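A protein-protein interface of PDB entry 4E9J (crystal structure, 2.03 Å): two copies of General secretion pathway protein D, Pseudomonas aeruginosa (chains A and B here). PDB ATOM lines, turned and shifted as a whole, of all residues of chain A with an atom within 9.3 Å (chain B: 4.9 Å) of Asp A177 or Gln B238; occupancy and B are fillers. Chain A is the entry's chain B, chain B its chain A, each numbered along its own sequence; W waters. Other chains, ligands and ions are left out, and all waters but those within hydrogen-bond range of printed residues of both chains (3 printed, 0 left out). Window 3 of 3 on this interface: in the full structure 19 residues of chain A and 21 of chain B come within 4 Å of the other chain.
The backbone carbonyl oxygen (O) of Tyr A178 is in hydrogen-bond range of the backbone NH (N) of Val B180, at 2.8 Å.
ND2 of Asn B182 lies within hydrogen-bond range of O of His A176.
The backbone NH (N) of Asn B182 sits at hydrogen-bond distance from the side-chain carboxylate (OD1) of Asp A177 (2.9 Å).
The side-chain amide nitrogen (NE2) of Gln B238 lies within hydrogen-bond range of the side-chain carboxylate (OD2) of Asp A177 (3.0 Å).
O of Gln B238 lies within hydrogen-bond range of OG1 of Thr B242, at 3.4 Å.
The side-chain carboxylate (OE1) of Glu A127 sits at hydrogen-bond distance from the backbone NH (N) of His A176, 2.7 Å away.
A ring nitrogen (NE2) of His A176 lies within hydrogen-bond range of the backbone carbonyl oxygen of Leu A170, 2.8 Å away.
The side-chain amide nitrogen (NE2) of Gln A172 sits close to a ring nitrogen (NE2) of His A176 (3.5 Å).
O of Asp A177 is in hydrogen-bond range of NE of Arg A230 (3.4 Å).
Among the printed residues, merely in contact across the chains: Asp A177 with Val B180 (3.4 Å), Asp A177 with Ile B181 (3.5 Å) and Ser A175 with Asn B182 (3.6 Å).
Printed residues of chain B within 4 Å of Ser A175: Asn B182.
Of the printed residues of chain B, His A176 touches Asn B182.
Of chain B, only Val B180, Ile B181, Asn B182 and Gln B238 come within 4 Å of Asp A177.
Printed residues of chain B within 4 Å of Tyr A178: Val B180 (2.8 Å).
Pro A226 touches none of the printed residues of chain B.
Pro A227 touches none of the printed residues of chain B.
Printed residues of chain A within 4 Å of Val B180: Asp A177 and Tyr A178.
Ile B181 touches just one residue of chain A: Asp A177.
Of chain A, only Ser A175, His A176 and Asp A177 come within 4 Å of Asn B182.
No residue of chain A comes within 4 Å of Ala B237.
The nearest residue of chain A that does not touch Gln B238 is Arg A230 (5.6 Å).
The nearest printed residue of chain B that does not touch Ser A175 is Ile B181 (7.0 Å).
Hydrophobic or aromatic side chains of chain B within 4 Å of the printed part of chain A: Val B180 and Ile B181.
Of the 22 printed residues of chain A, 4 touch a printed residue of chain B.
Along chain A the printed residues that touch a printed residue of chain B span positions 175 to 178.
Among the printed residues, no Asp or Glu carboxylate lies within 4 Å of a Lys or Arg side-chain nitrogen of the other chain.
Positions printed for both chains: 180 and 234.
Water W2 lies within hydrogen-bond range of the side-chain carboxylate (OD2) of Asp A177 (2.7 Å), the side-chain amide nitrogen (NE2) of Gln B238 (2.8 Å) and the guanidinium group (NH1) of Arg A230 (3.1 Å).
Water W3 lies within hydrogen-bond range of OD2 of Asp A177 (2.7 Å), NH2 of Arg A230 (2.9 Å) and NE2 of Gln B238 (3.5 Å).
Water W1 bridges O of Asn B182 and OG of Ser A175.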
ATOM      1  N   GLU A 127       1.423  22.091   4.270  1.00  0.00           N
ATOM      2  CA  GLU A 127       0.185  22.792   4.652  1.00  0.00           C
ATOM      3  C   GLU A 127       0.506  23.951   5.646  1.00  0.00           C
ATOM      4  O   GLU A 127      -0.141  25.003   5.601  1.00  0.00           O
ATOM      5  CB  GLU A 127      -0.793  21.833   5.307  1.00  0.00           C
ATOM      6  CG  GLU A 127      -2.161  22.470   5.517  1.00  0.00           C
ATOM      7  CD  GLU A 127      -3.230  21.619   6.181  1.00  0.00           C
ATOM      8  OE1 GLU A 127      -4.406  22.046   6.171  1.00  0.00           O
ATOM      9  OE2 GLU A 127      -2.895  20.560   6.754  1.00  0.00           O
ATOM     10  N   LEU A 131       0.856  29.190   6.360  1.00  0.00           N
ATOM     11  CA  LEU A 131       0.341  29.721   7.633  1.00  0.00           C
ATOM     12  C   LEU A 131       1.459  30.346   8.478  1.00  0.00           C
ATOM     13  O   LEU A 131       1.197  31.292   9.202  1.00  0.00           O
ATOM     14  CB  LEU A 131      -0.360  28.648   8.437  1.00  0.00           C
ATOM     15  CG  LEU A 131      -1.549  27.923   7.787  1.00  0.00           C
ATOM     16  CD1 LEU A 131      -1.988  26.800   8.627  1.00  0.00           C
ATOM     17  CD2 LEU A 131      -2.723  28.870   7.537  1.00  0.00           C
ATOM     18  N   LEU A 170      -0.502  24.647  16.198  1.00  0.00           N
ATOM     19  CA  LEU A 170      -1.105  24.226  14.925  1.00  0.00           C
ATOM     20  C   LEU A 170      -1.052  22.725  14.663  1.00  0.00           C
ATOM     21  O   LEU A 170      -1.953  22.178  14.021  1.00  0.00           O
ATOM     22  CB  LEU A 170      -0.362  24.914  13.755  1.00  0.00           C
ATOM     23  CG  LEU A 170      -0.632  26.399  13.514  1.00  0.00           C
ATOM     24  CD1 LEU A 170       0.415  26.973  12.619  1.00  0.00           C
ATOM     25  CD2 LEU A 170      -1.991  26.626  12.902  1.00  0.00           C
ATOM     26  N   GLN A 172      -1.460  19.116  14.118  1.00  0.00           N
ATOM     27  CA  GLN A 172      -2.630  18.243  14.275  1.00  0.00           C
ATOM     28  C   GLN A 172      -2.758  17.363  13.057  1.00  0.00           C
ATOM     29  O   GLN A 172      -2.213  17.676  11.987  1.00  0.00           O
ATOM     30  CB  GLN A 172      -3.922  19.032  14.507  1.00  0.00           C
ATOM     31  CG  GLN A 172      -4.394  19.826  13.281  1.00  0.00           C
ATOM     32  CD  GLN A 172      -5.607  20.670  13.586  1.00  0.00           C
ATOM     33  OE1 GLN A 172      -5.834  21.090  14.726  1.00  0.00           O
ATOM     34  NE2 GLN A 172      -6.429  20.923  12.573  1.00  0.00           N
ATOM     35  N   GLY A 174      -5.646  16.390  11.406  1.00  0.00           N
ATOM     36  CA  GLY A 174      -6.599  16.921  10.449  1.00  0.00           C
ATOM     37  C   GLY A 174      -6.138  18.174   9.729  1.00  0.00           C
ATOM     38  O   GLY A 174      -5.234  18.889  10.170  1.00  0.00           O
ATOM     39  N   SER A 175      -6.762  18.438   8.607  1.00  0.00           N
ATOM     40  CA  SER A 175      -6.448  19.609   7.786  1.00  0.00           C
ATOM     41  C   SER A 175      -6.903  20.903   8.478  1.00  0.00           C
ATOM     42  O   SER A 175      -7.804  20.885   9.304  1.00  0.00           O
ATOM     43  CB  SER A 175      -7.126  19.466   6.433  1.00  0.00           C
ATOM     44  OG  SER A 175      -6.624  18.285   5.831  1.00  0.00           O
ATOM     45  N   HIS A 176      -6.266  22.008   8.147  1.00  0.00           N
ATOM     46  CA  HIS A 176      -6.593  23.312   8.736  1.00  0.00           C
ATOM     47  C   HIS A 176      -7.475  24.126   7.812  1.00  0.00           C
ATOM     48  O   HIS A 176      -7.005  24.697   6.846  1.00  0.00           O
ATOM     49  CB  HIS A 176      -5.333  24.114   9.095  1.00  0.00           C
ATOM     50  CG  HIS A 176      -4.902  23.904  10.529  1.00  0.00           C
ATOM     51  ND1 HIS A 176      -5.676  24.370  11.589  1.00  0.00           N
ATOM     52  CD2 HIS A 176      -3.840  23.243  11.030  1.00  0.00           C
ATOM     53  CE1 HIS A 176      -5.038  24.026  12.688  1.00  0.00           C
ATOM     54  NE2 HIS A 176      -3.941  23.320  12.407  1.00  0.00           N
ATOM     55  N   ASP A 177      -8.773  24.117   8.077  1.00  0.00           N
ATOM     56  CA  ASP A 177      -9.680  25.006   7.390  1.00  0.00           C
ATOM     57  C   ASP A 177      -9.391  26.359   8.052  1.00  0.00           C
ATOM     58  O   ASP A 177      -9.073  26.406   9.237  1.00  0.00           O
ATOM     59  CB  ASP A 177     -11.153  24.619   7.635  1.00  0.00           C
ATOM     60  CG  ASP A 177     -11.622  23.446   6.792  1.00  0.00           C
ATOM     61  OD1 ASP A 177     -10.812  22.919   5.997  1.00  0.00           O
ATOM     62  OD2 ASP A 177     -12.816  23.120   6.850  1.00  0.00           O
ATOM     63  N   TYR A 178      -9.537  27.443   7.318  1.00  0.00           N
ATOM     64  CA  TYR A 178      -9.313  28.758   7.915  1.00  0.00           C
ATOM     65  C   TYR A 178     -10.032  29.846   7.226  1.00  0.00           C
ATOM     66  O   TYR A 178     -10.568  29.676   6.146  1.00  0.00           O
ATOM     67  CB  TYR A 178      -7.804  29.070   7.975  1.00  0.00           C
ATOM     68  CG  TYR A 178      -7.116  29.124   6.622  1.00  0.00           C
ATOM     69  CD1 TYR A 178      -6.993  30.322   5.925  1.00  0.00           C
ATOM     70  CD2 TYR A 178      -6.529  27.991   6.075  1.00  0.00           C
ATOM     71  CE1 TYR A 178      -6.296  30.386   4.712  1.00  0.00           C
ATOM     72  CE2 TYR A 178      -5.752  28.061   4.916  1.00  0.00           C
ATOM     73  CZ  TYR A 178      -5.690  29.242   4.204  1.00  0.00           C
ATOM     74  OH  TYR A 178      -5.012  29.220   3.008  1.00  0.00           O
ATOM     75  N   SER A 179     -10.048  30.986   7.878  1.00  0.00           N
ATOM     76  CA  SER A 179     -10.635  32.191   7.358  1.00  0.00           C
ATOM     77  C   SER A 179      -9.626  33.310   7.360  1.00  0.00           C
ATOM     78  O   SER A 179      -8.793  33.400   8.257  1.00  0.00           O
ATOM     79  CB  SER A 179     -11.869  32.570   8.157  1.00  0.00           C
ATOM     80  OG  SER A 179     -12.974  31.761   7.804  1.00  0.00           O
ATOM     81  N   VAL A 180      -9.687  34.164   6.321  1.00  0.00           N
ATOM     82  CA  VAL A 180      -8.827  35.325   6.171  1.00  0.00           C
ATOM     83  C   VAL A 180      -9.657  36.600   6.248  1.00  0.00           C
ATOM     84  O   VAL A 180     -10.672  36.706   5.570  1.00  0.00           O
ATOM     85  CB  VAL A 180      -8.024  35.230   4.859  1.00  0.00           C
ATOM     86  CG1 VAL A 180      -7.267  36.518   4.576  1.00  0.00           C
ATOM     87  CG2 VAL A 180      -7.083  34.038   4.892  1.00  0.00           C
ATOM     88  N   ALA A 210      -9.941  28.319  19.148  1.00  0.00           N
ATOM     89  CA  ALA A 210      -9.584  28.945  17.887  1.00  0.00           C
ATOM     90  C   ALA A 210      -8.219  29.606  18.024  1.00  0.00           C
ATOM     91  O   ALA A 210      -7.750  29.844  19.136  1.00  0.00           O
ATOM     92  CB  ALA A 210     -10.649  29.953  17.468  1.00  0.00           C
ATOM     93  N   GLN A 211      -7.563  29.836  16.900  1.00  0.00           N
ATOM     94  CA  GLN A 211      -6.211  30.413  16.862  1.00  0.00           C
ATOM     95  C   GLN A 211      -6.164  31.517  15.816  1.00  0.00           C
ATOM     96  O   GLN A 211      -6.813  31.408  14.782  1.00  0.00           O
ATOM     97  CB  GLN A 211      -5.156  29.318  16.562  1.00  0.00           C
ATOM     98  CG  GLN A 211      -3.731  29.815  16.363  1.00  0.00           C
ATOM     99  CD  GLN A 211      -2.735  28.698  16.253  1.00  0.00           C
ATOM    100  OE1 GLN A 211      -3.080  27.516  16.202  1.00  0.00           O
ATOM    101  NE2 GLN A 211      -1.458  29.045  16.239  1.00  0.00           N
ATOM    102  N   ILE A 222      -5.424  35.558   9.978  1.00  0.00           N
ATOM    103  CA  ILE A 222      -5.714  34.194   9.546  1.00  0.00           C
ATOM    104  C   ILE A 222      -6.276  33.536  10.803  1.00  0.00           C
ATOM    105  O   ILE A 222      -5.590  33.534  11.827  1.00  0.00           O
ATOM    106  CB  ILE A 222      -4.473  33.498   9.008  1.00  0.00           C
ATOM    107  CG1 ILE A 222      -3.940  34.230   7.757  1.00  0.00           C
ATOM    108  CG2 ILE A 222      -4.770  32.041   8.729  1.00  0.00           C
ATOM    109  CD1 ILE A 222      -2.469  33.919   7.437  1.00  0.00           C
ATOM    110  N   ILE A 223      -7.542  33.082  10.749  1.00  0.00           N
ATOM    111  CA  ILE A 223      -8.307  32.472  11.850  1.00  0.00           C
ATOM    112  C   ILE A 223      -8.506  30.955  11.636  1.00  0.00           C
ATOM    113  O   ILE A 223      -9.143  30.553  10.665  1.00  0.00           O
ATOM    114  CB  ILE A 223      -9.702  33.185  11.980  1.00  0.00           C
ATOM    115  CG1 ILE A 223      -9.589  34.754  12.016  1.00  0.00           C
ATOM    116  CG2 ILE A 223     -10.432  32.663  13.164  1.00  0.00           C
ATOM    117  CD1 ILE A 223      -9.120  35.335  13.257  1.00  0.00           C
ATOM    118  N   LEU A 224      -7.968  30.137  12.551  1.00  0.00           N
ATOM    119  CA  LEU A 224      -7.966  28.679  12.505  1.00  0.00           C
ATOM    120  C   LEU A 224      -8.760  28.133  13.667  1.00  0.00           C
ATOM    121  O   LEU A 224      -8.976  28.855  14.629  1.00  0.00           O
ATOM    122  CB  LEU A 224      -6.519  28.153  12.769  1.00  0.00           C
ATOM    123  CG  LEU A 224      -5.291  28.534  11.902  1.00  0.00           C
ATOM    124  CD1 LEU A 224      -5.444  28.155  10.504  1.00  0.00           C
ATOM    125  CD2 LEU A 224      -4.870  29.954  12.069  1.00  0.00           C
ATOM    126  N   GLY A 225      -8.985  26.814  13.659  1.00  0.00           N
ATOM    127  CA  GLY A 225      -9.527  26.078  14.803  1.00  0.00           C
ATOM    128  C   GLY A 225     -10.632  25.120  14.422  1.00  0.00           C
ATOM    129  O   GLY A 225     -10.974  24.984  13.249  1.00  0.00           O
ATOM    130  N   PRO A 226     -11.226  24.454  15.423  1.00  0.00           N
ATOM    131  CA  PRO A 226     -12.387  23.591  15.139  1.00  0.00           C
ATOM    132  C   PRO A 226     -13.568  24.453  14.640  1.00  0.00           C
ATOM    133  O   PRO A 226     -13.579  25.677  14.865  1.00  0.00           O
ATOM    134  CB  PRO A 226     -12.637  22.879  16.467  1.00  0.00           C
ATOM    135  CG  PRO A 226     -11.993  23.666  17.467  1.00  0.00           C
ATOM    136  CD  PRO A 226     -10.912  24.485  16.862  1.00  0.00           C
ATOM    137  N   PRO A 227     -14.503  23.875  13.867  1.00  0.00           N
ATOM    138  CA  PRO A 227     -15.497  24.707  13.179  1.00  0.00           C
ATOM    139  C   PRO A 227     -16.265  25.757  13.977  1.00  0.00           C
ATOM    140  O   PRO A 227     -16.370  26.898  13.533  1.00  0.00           O
ATOM    141  CB  PRO A 227     -16.452  23.688  12.543  1.00  0.00           C
ATOM    142  CG  PRO A 227     -15.706  22.428  12.489  1.00  0.00           C
ATOM    143  CD  PRO A 227     -14.591  22.461  13.451  1.00  0.00           C
ATOM    144  N   ARG A 230     -13.842  28.446  15.516  1.00  0.00           N
ATOM    145  CA  ARG A 230     -13.330  29.264  14.404  1.00  0.00           C
ATOM    146  C   ARG A 230     -14.390  30.241  13.877  1.00  0.00           C
ATOM    147  O   ARG A 230     -14.121  31.446  13.725  1.00  0.00           O
ATOM    148  CB  ARG A 230     -12.834  28.346  13.278  1.00  0.00           C
ATOM    149  CG  ARG A 230     -12.537  29.023  11.953  1.00  0.00           C
ATOM    150  CD  ARG A 230     -11.585  28.194  11.100  1.00  0.00           C
ATOM    151  NE  ARG A 230     -11.811  26.756  11.244  1.00  0.00           N
ATOM    152  CZ  ARG A 230     -12.679  26.014  10.559  1.00  0.00           C
ATOM    153  NH1 ARG A 230     -13.440  26.558   9.619  1.00  0.00           N
ATOM    154  NH2 ARG A 230     -12.799  24.723  10.818  1.00  0.00           N
ATOM    155  N   ALA A 231     -15.600  29.757  13.638  1.00  0.00           N
ATOM    156  CA  ALA A 231     -16.681  30.618  13.131  1.00  0.00           C
ATOM    157  C   ALA A 231     -16.993  31.760  14.107  1.00  0.00           C
ATOM    158  O   ALA A 231     -17.266  32.884  13.683  1.00  0.00           O
ATOM    159  CB  ALA A 231     -17.933  29.785  12.873  1.00  0.00           C
ATOM    160  N   VAL A 234     -14.087  34.426  14.023  1.00  0.00           N
ATOM    161  CA  VAL A 234     -14.238  35.263  12.802  1.00  0.00           C
ATOM    162  C   VAL A 234     -15.232  36.404  13.113  1.00  0.00           C
ATOM    163  O   VAL A 234     -14.947  37.542  12.792  1.00  0.00           O
ATOM    164  CB  VAL A 234     -14.638  34.447  11.553  1.00  0.00           C
ATOM    165  CG1 VAL A 234     -15.022  35.384  10.394  1.00  0.00           C
ATOM    166  CG2 VAL A 234     -13.481  33.542  11.117  1.00  0.00           C
ATOM    167  N   VAL B 180     -11.439  28.951   3.581  1.00  0.00           N
ATOM    168  CA  VAL B 180     -10.853  27.786   2.931  1.00  0.00           C
ATOM    169  C   VAL B 180     -11.391  26.494   3.557  1.00  0.00           C
ATOM    170  O   VAL B 180     -11.394  26.364   4.782  1.00  0.00           O
ATOM    171  CB  VAL B 180      -9.327  27.868   3.027  1.00  0.00           C
ATOM    172  CG1 VAL B 180      -8.685  26.579   2.545  1.00  0.00           C
ATOM    173  CG2 VAL B 180      -8.813  29.078   2.261  1.00  0.00           C
ATOM    174  N   ILE B 181     -11.840  25.544   2.696  1.00  0.00           N
ATOM    175  CA  ILE B 181     -12.338  24.226   3.100  1.00  0.00           C
ATOM    176  C   ILE B 181     -11.540  23.153   2.403  1.00  0.00           C
ATOM    177  O   ILE B 181     -11.614  23.050   1.186  1.00  0.00           O
ATOM    178  CB  ILE B 181     -13.819  24.029   2.809  1.00  0.00           C
ATOM    179  CG1 ILE B 181     -14.646  25.096   3.466  1.00  0.00           C
ATOM    180  CG2 ILE B 181     -14.286  22.611   3.264  1.00  0.00           C
ATOM    181  CD1 ILE B 181     -16.017  25.128   2.952  1.00  0.00           C
ATOM    182  N   ASN B 182     -10.835  22.334   3.167  1.00  0.00           N
ATOM    183  CA  ASN B 182     -10.042  21.213   2.669  1.00  0.00           C
ATOM    184  C   ASN B 182     -10.989  20.038   2.609  1.00  0.00           C
ATOM    185  O   ASN B 182     -11.416  19.570   3.636  1.00  0.00           O
ATOM    186  CB  ASN B 182      -8.908  20.910   3.630  1.00  0.00           C
ATOM    187  CG  ASN B 182      -7.989  22.074   3.774  1.00  0.00           C
ATOM    188  OD1 ASN B 182      -7.148  22.302   2.938  1.00  0.00           O
ATOM    189  ND2 ASN B 182      -8.173  22.877   4.802  1.00  0.00           N
ATOM    190  N   VAL B 234     -20.125  28.556   3.271  1.00  0.00           N
ATOM    191  CA  VAL B 234     -19.187  27.687   4.007  1.00  0.00           C
ATOM    192  C   VAL B 234     -19.973  26.513   4.644  1.00  0.00           C
ATOM    193  O   VAL B 234     -19.561  25.361   4.520  1.00  0.00           O
ATOM    194  CB  VAL B 234     -18.321  28.459   5.038  1.00  0.00           C
ATOM    195  CG1 VAL B 234     -17.539  27.515   5.943  1.00  0.00           C
ATOM    196  CG2 VAL B 234     -17.359  29.414   4.328  1.00  0.00           C
ATOM    197  N   GLN B 235     -21.127  26.802   5.270  1.00  0.00           N
ATOM    198  CA  GLN B 235     -21.961  25.756   5.873  1.00  0.00           C
ATOM    199  C   GLN B 235     -22.470  24.788   4.810  1.00  0.00           C
ATOM    200  O   GLN B 235     -22.388  23.586   5.013  1.00  0.00           O
ATOM    201  CB  GLN B 235     -23.152  26.366   6.649  1.00  0.00           C
ATOM    202  N   LEU B 236     -22.974  25.318   3.678  1.00  0.00           N
ATOM    203  CA  LEU B 236     -23.460  24.524   2.537  1.00  0.00           C
ATOM    204  C   LEU B 236     -22.350  23.629   1.980  1.00  0.00           C
ATOM    205  O   LEU B 236     -22.626  22.481   1.656  1.00  0.00           O
ATOM    206  CB  LEU B 236     -23.983  25.433   1.407  1.00  0.00           C
ATOM    207  CG  LEU B 236     -24.732  24.701   0.260  1.00  0.00           C
ATOM    208  CD1 LEU B 236     -26.052  24.101   0.743  1.00  0.00           C
ATOM    209  CD2 LEU B 236     -25.004  25.628  -0.920  1.00  0.00           C
ATOM    210  N   ALA B 237     -21.123  24.173   1.813  1.00  0.00           N
ATOM    211  CA  ALA B 237     -19.955  23.407   1.341  1.00  0.00           C
ATOM    212  C   ALA B 237     -19.631  22.256   2.278  1.00  0.00           C
ATOM    213  O   ALA B 237     -19.355  21.143   1.810  1.00  0.00           O
ATOM    214  CB  ALA B 237     -18.753  24.316   1.190  1.00  0.00           C
ATOM    215  N   GLN B 238     -19.765  22.463   3.585  1.00  0.00           N
ATOM    216  CA  GLN B 238     -19.509  21.379   4.522  1.00  0.00           C
ATOM    217  C   GLN B 238     -20.489  20.210   4.384  1.00  0.00           C
ATOM    218  O   GLN B 238     -20.047  19.067   4.471  1.00  0.00           O
ATOM    219  CB  GLN B 238     -19.363  21.916   5.952  1.00  0.00           C
ATOM    220  CG  GLN B 238     -18.079  22.761   6.127  1.00  0.00           C
ATOM    221  CD  GLN B 238     -16.814  21.957   6.078  1.00  0.00           C
ATOM    222  OE1 GLN B 238     -16.831  20.737   5.900  1.00  0.00           O
ATOM    223  NE2 GLN B 238     -15.676  22.630   6.249  1.00  0.00           N
ATOM    224  N   SER B 239     -21.754  20.469   3.975  1.00  0.00           N
ATOM    225  CA  SER B 239     -22.726  19.396   3.735  1.00  0.00           C
ATOM    226  C   SER B 239     -22.397  18.520   2.505  1.00  0.00           C
ATOM    227  O   SER B 239     -22.919  17.417   2.409  1.00  0.00           O
ATOM    228  CB  SER B 239     -24.148  19.958   3.624  1.00  0.00           C
ATOM    229  OG  SER B 239     -24.425  20.530   2.353  1.00  0.00           O
ATOM    230  N   LEU B 240     -21.581  19.005   1.553  1.00  0.00           N
ATOM    231  CA  LEU B 240     -21.186  18.217   0.381  1.00  0.00           C
ATOM    232  C   LEU B 240     -20.004  17.309   0.683  1.00  0.00           C
ATOM    233  O   LEU B 240     -19.741  16.387  -0.085  1.00  0.00           O
ATOM    234  CB  LEU B 240     -20.819  19.125  -0.802  1.00  0.00           C
ATOM    235  CG  LEU B 240     -21.893  20.127  -1.227  1.00  0.00           C
ATOM    236  CD1 LEU B 240     -21.404  20.960  -2.410  1.00  0.00           C
ATOM    237  CD2 LEU B 240     -23.228  19.434  -1.552  1.00  0.00           C
ATOM    238  N   ASP B 241     -19.283  17.571   1.774  1.00  0.00           N
ATOM    239  CA  ASP B 241     -18.155  16.757   2.194  1.00  0.00           C
ATOM    240  C   ASP B 241     -18.498  15.894   3.411  1.00  0.00           C
ATOM    241  O   ASP B 241     -17.683  15.732   4.302  1.00  0.00           O
ATOM    242  CB  ASP B 241     -16.968  17.688   2.476  1.00  0.00           C
ATOM    243  CG  ASP B 241     -15.634  16.993   2.501  1.00  0.00           C
ATOM    244  OD1 ASP B 241     -15.358  16.186   1.583  1.00  0.00           O
ATOM    245  OD2 ASP B 241     -14.837  17.297   3.396  1.00  0.00           O
ATOM    246  N   THR B 242     -19.744  15.360   3.445  1.00  0.00           N
ATOM    247  CA  THR B 242     -20.276  14.522   4.532  1.00  0.00           C
ATOM    248  C   THR B 242     -20.078  13.054   4.172  1.00  0.00           C
ATOM    249  O   THR B 242     -19.405  12.335   4.905  1.00  0.00           O
ATOM    250  CB  THR B 242     -21.759  14.885   4.786  1.00  0.00           C
ATOM    251  OG1 THR B 242     -21.832  16.238   5.243  1.00  0.00           O
ATOM    252  CG2 THR B 242     -22.441  13.964   5.807  1.00  0.00           C
HETATM  253  O   HOH W   1     -10.008  17.665   5.479  1.00  0.00           O
HETATM  254  O   HOH W   2     -14.644  25.017   7.239  1.00  0.00           O
HETATM  255  O   HOH W   3     -13.920  22.480   9.266  1.00  0.00           O
